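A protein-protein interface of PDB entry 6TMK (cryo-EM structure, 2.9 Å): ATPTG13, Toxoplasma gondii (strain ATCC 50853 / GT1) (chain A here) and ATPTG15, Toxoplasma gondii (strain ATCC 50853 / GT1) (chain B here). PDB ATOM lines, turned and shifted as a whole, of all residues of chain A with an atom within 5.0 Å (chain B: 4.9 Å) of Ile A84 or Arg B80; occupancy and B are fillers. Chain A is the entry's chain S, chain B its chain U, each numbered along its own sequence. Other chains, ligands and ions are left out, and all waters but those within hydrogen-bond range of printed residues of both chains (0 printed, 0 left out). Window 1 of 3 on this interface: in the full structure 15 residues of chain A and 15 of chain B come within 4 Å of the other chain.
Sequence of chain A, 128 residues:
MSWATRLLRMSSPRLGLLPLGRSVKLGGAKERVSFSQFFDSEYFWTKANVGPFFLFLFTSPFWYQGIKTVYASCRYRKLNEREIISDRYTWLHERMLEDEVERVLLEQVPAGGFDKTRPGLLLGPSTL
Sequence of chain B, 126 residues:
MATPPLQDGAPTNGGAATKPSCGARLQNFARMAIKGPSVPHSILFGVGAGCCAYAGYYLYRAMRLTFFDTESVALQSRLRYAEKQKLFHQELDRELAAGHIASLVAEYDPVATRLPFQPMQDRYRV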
ATOM      1  N   LEU A  79      29.598  20.077 -10.602  1.00  0.00           N
ATOM      2  CA  LEU A  79      28.633  20.050 -11.689  1.00  0.00           C
ATOM      3  C   LEU A  79      28.659  18.717 -12.418  1.00  0.00           C
ATOM      4  O   LEU A  79      27.614  18.214 -12.834  1.00  0.00           O
ATOM      5  CB  LEU A  79      28.919  21.200 -12.644  1.00  0.00           C
ATOM      6  CG  LEU A  79      28.104  21.266 -13.922  1.00  0.00           C
ATOM      7  CD1 LEU A  79      26.653  21.521 -13.625  1.00  0.00           C
ATOM      8  CD2 LEU A  79      28.670  22.359 -14.765  1.00  0.00           C
ATOM      9  N   ASN A  80      29.845  18.145 -12.609  1.00  0.00           N
ATOM     10  CA  ASN A  80      29.950  16.841 -13.244  1.00  0.00           C
ATOM     11  C   ASN A  80      29.233  15.785 -12.416  1.00  0.00           C
ATOM     12  O   ASN A  80      28.477  14.957 -12.948  1.00  0.00           O
ATOM     13  CB  ASN A  80      31.425  16.492 -13.415  1.00  0.00           C
ATOM     14  CG  ASN A  80      31.648  15.306 -14.309  1.00  0.00           C
ATOM     15  OD1 ASN A  80      31.093  15.216 -15.401  1.00  0.00           O
ATOM     16  ND2 ASN A  80      32.472  14.384 -13.850  1.00  0.00           N
ATOM     17  N   GLU A  81      29.456  15.807 -11.101  1.00  0.00           N
ATOM     18  CA  GLU A  81      28.742  14.891 -10.215  1.00  0.00           C
ATOM     19  C   GLU A  81      27.231  15.034 -10.375  1.00  0.00           C
ATOM     20  O   GLU A  81      26.507  14.043 -10.583  1.00  0.00           O
ATOM     21  CB  GLU A  81      29.157  15.147  -8.771  1.00  0.00           C
ATOM     22  CG  GLU A  81      28.653  14.129  -7.787  1.00  0.00           C
ATOM     23  CD  GLU A  81      29.369  14.209  -6.456  1.00  0.00           C
ATOM     24  OE1 GLU A  81      30.566  13.856  -6.402  1.00  0.00           O
ATOM     25  OE2 GLU A  81      28.739  14.629  -5.464  1.00  0.00           O
ATOM     26  N   ARG A  82      26.740  16.272 -10.289  1.00  0.00           N
ATOM     27  CA  ARG A  82      25.306  16.511 -10.383  1.00  0.00           C
ATOM     28  C   ARG A  82      24.753  16.061 -11.726  1.00  0.00           C
ATOM     29  O   ARG A  82      23.664  15.484 -11.792  1.00  0.00           O
ATOM     30  CB  ARG A  82      25.006  17.989 -10.153  1.00  0.00           C
ATOM     31  CG  ARG A  82      23.540  18.333 -10.277  1.00  0.00           C
ATOM     32  CD  ARG A  82      23.187  19.594  -9.536  1.00  0.00           C
ATOM     33  NE  ARG A  82      21.748  19.826  -9.532  1.00  0.00           N
ATOM     34  CZ  ARG A  82      21.180  20.985  -9.229  1.00  0.00           C
ATOM     35  NH1 ARG A  82      21.925  22.027  -8.907  1.00  0.00           N
ATOM     36  NH2 ARG A  82      19.863  21.102  -9.252  1.00  0.00           N
ATOM     37  N   GLU A  83      25.485  16.317 -12.807  1.00  0.00           N
ATOM     38  CA  GLU A  83      25.005  15.958 -14.133  1.00  0.00           C
ATOM     39  C   GLU A  83      24.893  14.450 -14.286  1.00  0.00           C
ATOM     40  O   GLU A  83      23.902  13.945 -14.833  1.00  0.00           O
ATOM     41  CB  GLU A  83      25.943  16.533 -15.190  1.00  0.00           C
ATOM     42  CG  GLU A  83      25.345  16.594 -16.575  1.00  0.00           C
ATOM     43  CD  GLU A  83      26.388  16.617 -17.678  1.00  0.00           C
ATOM     44  OE1 GLU A  83      27.539  16.202 -17.430  1.00  0.00           O
ATOM     45  OE2 GLU A  83      26.052  17.047 -18.803  1.00  0.00           O
ATOM     46  N   ILE A  84      25.896  13.713 -13.811  1.00  0.00           N
ATOM     47  CA  ILE A  84      25.831  12.256 -13.885  1.00  0.00           C
ATOM     48  C   ILE A  84      24.611  11.743 -13.130  1.00  0.00           C
ATOM     49  O   ILE A  84      23.826  10.933 -13.649  1.00  0.00           O
ATOM     50  CB  ILE A  84      27.131  11.634 -13.351  1.00  0.00           C
ATOM     51  CG1 ILE A  84      28.285  11.969 -14.281  1.00  0.00           C
ATOM     52  CG2 ILE A  84      26.992  10.151 -13.230  1.00  0.00           C
ATOM     53  CD1 ILE A  84      29.616  11.809 -13.679  1.00  0.00           C
ATOM     54  N   ILE A  85      24.435  12.205 -11.891  1.00  0.00           N
ATOM     55  CA  ILE A  85      23.333  11.682 -11.090  1.00  0.00           C
ATOM     56  C   ILE A  85      21.987  12.078 -11.682  1.00  0.00           C
ATOM     57  O   ILE A  85      21.025  11.303 -11.630  1.00  0.00           O
ATOM     58  CB  ILE A  85      23.482  12.138  -9.631  1.00  0.00           C
ATOM     59  CG1 ILE A  85      24.728  11.499  -9.034  1.00  0.00           C
ATOM     60  CG2 ILE A  85      22.254  11.782  -8.833  1.00  0.00           C
ATOM     61  CD1 ILE A  85      25.148  12.077  -7.745  1.00  0.00           C
ATOM     62  N   SER A  86      21.902  13.260 -12.286  1.00  0.00           N
ATOM     63  CA  SER A  86      20.662  13.705 -12.909  1.00  0.00           C
ATOM     64  C   SER A  86      20.308  12.829 -14.101  1.00  0.00           C
ATOM     65  O   SER A  86      19.149  12.420 -14.269  1.00  0.00           O
ATOM     66  CB  SER A  86      20.801  15.167 -13.316  1.00  0.00           C
ATOM     67  OG  SER A  86      19.678  15.620 -14.041  1.00  0.00           O
ATOM     68  N   ASP A  87      21.290  12.540 -14.951  1.00  0.00           N
ATOM     69  CA  ASP A  87      21.027  11.694 -16.105  1.00  0.00           C
ATOM     70  C   ASP A  87      20.593  10.304 -15.668  1.00  0.00           C
ATOM     71  O   ASP A  87      19.680   9.711 -16.261  1.00  0.00           O
ATOM     72  CB  ASP A  87      22.269  11.627 -16.988  1.00  0.00           C
ATOM     73  CG  ASP A  87      22.049  10.823 -18.253  1.00  0.00           C
ATOM     74  OD1 ASP A  87      22.647   9.731 -18.378  1.00  0.00           O
ATOM     75  OD2 ASP A  87      21.284  11.287 -19.127  1.00  0.00           O
ATOM     76  N   ARG A  88      21.213   9.775 -14.614  1.00  0.00           N
ATOM     77  CA  ARG A  88      20.824   8.452 -14.140  1.00  0.00           C
ATOM     78  C   ARG A  88      19.429   8.458 -13.524  1.00  0.00           C
ATOM     79  O   ARG A  88      18.690   7.476 -13.662  1.00  0.00           O
ATOM     80  CB  ARG A  88      21.860   7.937 -13.157  1.00  0.00           C
ATOM     81  CG  ARG A  88      23.133   7.562 -13.829  1.00  0.00           C
ATOM     82  CD  ARG A  88      24.154   7.051 -12.878  1.00  0.00           C
ATOM     83  NE  ARG A  88      25.398   6.728 -13.559  1.00  0.00           N
ATOM     84  CZ  ARG A  88      26.484   6.282 -12.947  1.00  0.00           C
ATOM     85  NH1 ARG A  88      26.475   6.098 -11.642  1.00  0.00           N
ATOM     86  NH2 ARG A  88      27.572   6.015 -13.642  1.00  0.00           N
ATOM     87  N   VAL B  73      36.738  17.489 -17.054  1.00  0.00           N
ATOM     88  CA  VAL B  73      35.298  17.444 -16.832  1.00  0.00           C
ATOM     89  C   VAL B  73      34.556  17.717 -18.131  1.00  0.00           C
ATOM     90  O   VAL B  73      33.593  17.019 -18.481  1.00  0.00           O
ATOM     91  CB  VAL B  73      34.903  18.450 -15.738  1.00  0.00           C
ATOM     92  CG1 VAL B  73      33.410  18.672 -15.719  1.00  0.00           C
ATOM     93  CG2 VAL B  73      35.379  17.968 -14.404  1.00  0.00           C
ATOM     94  N   GLN B  76      34.863  14.707 -20.384  1.00  0.00           N
ATOM     95  CA  GLN B  76      34.051  13.601 -19.897  1.00  0.00           C
ATOM     96  C   GLN B  76      32.589  13.801 -20.270  1.00  0.00           C
ATOM     97  O   GLN B  76      31.914  12.873 -20.737  1.00  0.00           O
ATOM     98  CB  GLN B  76      34.217  13.481 -18.387  1.00  0.00           C
ATOM     99  CG  GLN B  76      35.501  12.821 -17.964  1.00  0.00           C
ATOM    100  CD  GLN B  76      35.697  12.847 -16.466  1.00  0.00           C
ATOM    101  OE1 GLN B  76      34.763  13.101 -15.710  1.00  0.00           O
ATOM    102  NE2 GLN B  76      36.922  12.599 -16.028  1.00  0.00           N
ATOM    103  N   SER B  77      32.082  15.015 -20.060  1.00  0.00           N
ATOM    104  CA  SER B  77      30.715  15.330 -20.452  1.00  0.00           C
ATOM    105  C   SER B  77      30.519  15.108 -21.944  1.00  0.00           C
ATOM    106  O   SER B  77      29.537  14.487 -22.376  1.00  0.00           O
ATOM    107  CB  SER B  77      30.397  16.772 -20.063  1.00  0.00           C
ATOM    108  OG  SER B  77      29.006  17.017 -20.034  1.00  0.00           O
ATOM    109  N   ARG B  78      31.454  15.611 -22.748  1.00  0.00           N
ATOM    110  CA  ARG B  78      31.343  15.474 -24.190  1.00  0.00           C
ATOM    111  C   ARG B  78      31.414  14.016 -24.627  1.00  0.00           C
ATOM    112  O   ARG B  78      30.747  13.623 -25.590  1.00  0.00           O
ATOM    113  CB  ARG B  78      32.441  16.304 -24.844  1.00  0.00           C
ATOM    114  CG  ARG B  78      32.349  16.449 -26.327  1.00  0.00           C
ATOM    115  CD  ARG B  78      31.064  17.056 -26.768  1.00  0.00           C
ATOM    116  NE  ARG B  78      31.037  17.237 -28.209  1.00  0.00           N
ATOM    117  CZ  ARG B  78      29.933  17.431 -28.908  1.00  0.00           C
ATOM    118  NH1 ARG B  78      28.768  17.486 -28.310  1.00  0.00           N
ATOM    119  NH2 ARG B  78      29.998  17.575 -30.207  1.00  0.00           N
ATOM    120  N   LEU B  79      32.172  13.191 -23.911  1.00  0.00           N
ATOM    121  CA  LEU B  79      32.281  11.785 -24.274  1.00  0.00           C
ATOM    122  C   LEU B  79      31.019  11.017 -23.907  1.00  0.00           C
ATOM    123  O   LEU B  79      30.607  10.103 -24.632  1.00  0.00           O
ATOM    124  CB  LEU B  79      33.505  11.178 -23.602  1.00  0.00           C
ATOM    125  CG  LEU B  79      34.840  11.658 -24.167  1.00  0.00           C
ATOM    126  CD1 LEU B  79      35.979  11.239 -23.281  1.00  0.00           C
ATOM    127  CD2 LEU B  79      35.062  11.168 -25.564  1.00  0.00           C
ATOM    128  N   ARG B  80      30.389  11.369 -22.789  1.00  0.00           N
ATOM    129  CA  ARG B  80      29.087  10.794 -22.469  1.00  0.00           C
ATOM    130  C   ARG B  80      28.046  11.158 -23.523  1.00  0.00           C
ATOM    131  O   ARG B  80      27.244  10.313 -23.952  1.00  0.00           O
ATOM    132  CB  ARG B  80      28.657  11.266 -21.085  1.00  0.00           C
ATOM    133  CG  ARG B  80      29.501  10.709 -19.975  1.00  0.00           C
ATOM    134  CD  ARG B  80      28.954  11.074 -18.626  1.00  0.00           C
ATOM    135  NE  ARG B  80      29.663  12.197 -18.018  1.00  0.00           N
ATOM    136  CZ  ARG B  80      29.097  13.325 -17.610  1.00  0.00           C
ATOM    137  NH1 ARG B  80      27.799  13.537 -17.742  1.00  0.00           N
ATOM    138  NH2 ARG B  80      29.851  14.256 -17.066  1.00  0.00           N
ATOM    139  N   TYR B  81      28.048  12.421 -23.945  1.00  0.00           N
ATOM    140  CA  TYR B  81      27.205  12.849 -25.055  1.00  0.00           C
ATOM    141  C   TYR B  81      27.470  12.008 -26.299  1.00  0.00           C
ATOM    142  O   TYR B  81      26.534  11.572 -26.985  1.00  0.00           O
ATOM    143  CB  TYR B  81      27.466  14.330 -25.314  1.00  0.00           C
ATOM    144  CG  TYR B  81      26.604  14.996 -26.348  1.00  0.00           C
ATOM    145  CD1 TYR B  81      25.468  15.678 -25.976  1.00  0.00           C
ATOM    146  CD2 TYR B  81      26.941  14.977 -27.685  1.00  0.00           C
ATOM    147  CE1 TYR B  81      24.689  16.301 -26.897  1.00  0.00           C
ATOM    148  CE2 TYR B  81      26.165  15.596 -28.610  1.00  0.00           C
ATOM    149  CZ  TYR B  81      25.039  16.260 -28.214  1.00  0.00           C
ATOM    150  OH  TYR B  81      24.257  16.886 -29.148  1.00  0.00           O
ATOM    151  N   ALA B  82      28.746  11.763 -26.598  1.00  0.00           N
ATOM    152  CA  ALA B  82      29.104  10.960 -27.757  1.00  0.00           C
ATOM    153  C   ALA B  82      28.581   9.538 -27.628  1.00  0.00           C
ATOM    154  O   ALA B  82      28.169   8.930 -28.620  1.00  0.00           O
ATOM    155  CB  ALA B  82      30.616  10.961 -27.928  1.00  0.00           C
ATOM    156  N   GLU B  83      28.615   8.981 -26.421  1.00  0.00           N
ATOM    157  CA  GLU B  83      28.090   7.637 -26.213  1.00  0.00           C
ATOM    158  C   GLU B  83      26.600   7.580 -26.516  1.00  0.00           C
ATOM    159  O   GLU B  83      26.121   6.664 -27.200  1.00  0.00           O
ATOM    160  CB  GLU B  83      28.356   7.199 -24.781  1.00  0.00           C
ATOM    161  CG  GLU B  83      28.334   5.711 -24.589  1.00  0.00           C
ATOM    162  CD  GLU B  83      28.211   5.323 -23.139  1.00  0.00           C
ATOM    163  OE1 GLU B  83      28.457   6.184 -22.272  1.00  0.00           O
ATOM    164  OE2 GLU B  83      27.865   4.158 -22.863  1.00  0.00           O
ATOM    165  N   LYS B  84      25.844   8.545 -25.991  1.00  0.00           N
ATOM    166  CA  LYS B  84      24.418   8.606 -26.289  1.00  0.00           C
ATOM    167  C   LYS B  84      24.175   8.683 -27.791  1.00  0.00           C
ATOM    168  O   LYS B  84      23.318   7.976 -28.338  1.00  0.00           O
ATOM    169  CB  LYS B  84      23.800   9.802 -25.578  1.00  0.00           C
ATOM    170  CG  LYS B  84      23.693   9.630 -24.107  1.00  0.00           C
ATOM    171  CD  LYS B  84      23.160  10.860 -23.440  1.00  0.00           C
ATOM    172  CE  LYS B  84      23.185  10.716 -21.936  1.00  0.00           C
ATOM    173  NZ  LYS B  84      24.418  11.294 -21.335  1.00  0.00           N
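Hydrophobic or aromatic side chains of chain A within 4 Å of the printed part of chain B: Ile A84.
Of the 10 printed residues of chain B, 5 touch a printed residue of chain A.
Printed residues of chain B that touch a printed residue of chain A: Val B73, Gln B76, Ser B77, Arg B80 and Lys B84.
Hydrophobic or aromatic side chains of chain B within 4 Å of the printed part of chain A: Val B73.
Of the printed residues of chain B, Asn A80 touches Val B73 (3.7 Å), Gln B76 (3.2 Å) and Arg B80 (2.3 Å).
Of the printed residues of chain B, Ile A84 touches Arg B80 (3.7 Å).
Arg A88 touches none of the printed residues of chain B.
Printed residues of chain A within 4 Å of Val B73: Asn A80.
Of the printed residues of chain A, Gln B76 touches Asn A80.
Of the printed residues of chain A, Ser B77 touches Glu A83 (3.1 Å).
Arg B80 touches just these residues of chain A: Asn A80 (2.3 Å), Glu A83 (2.7 Å) and Ile A84 (3.7 Å).
The nearest printed residue of chain A that does not touch Arg B80 is Asp A87 (5.9 Å).
The nearest printed residue of chain A that does not touch Gln B76 is Ile A84 (5.7 Å).
CB of Asn A80 touches CG1 of Val B73, 3.7 Å away.
Ile A84 touches Arg B80.
ND2 of Asn A80 lies within hydrogen-bond range of OE1 of Gln B76 (3.2 Å).
OD1 of Asp A87 lies within salt-bridge range of NZ of Lys B84.
The side-chain carboxylate (OE1) of Glu A83 is in hydrogen-bond range of the side-chain hydroxyl (OG) of Ser B77 (3.1 Å).
The guanidinium group (NH1) of Arg B80 lies within salt-bridge range of the side-chain carboxylate (OE1) of Glu A83 (2.7 Å).
NH2 of Arg B80 lies close to OD1 of Asn A80, at 2.3 Å.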
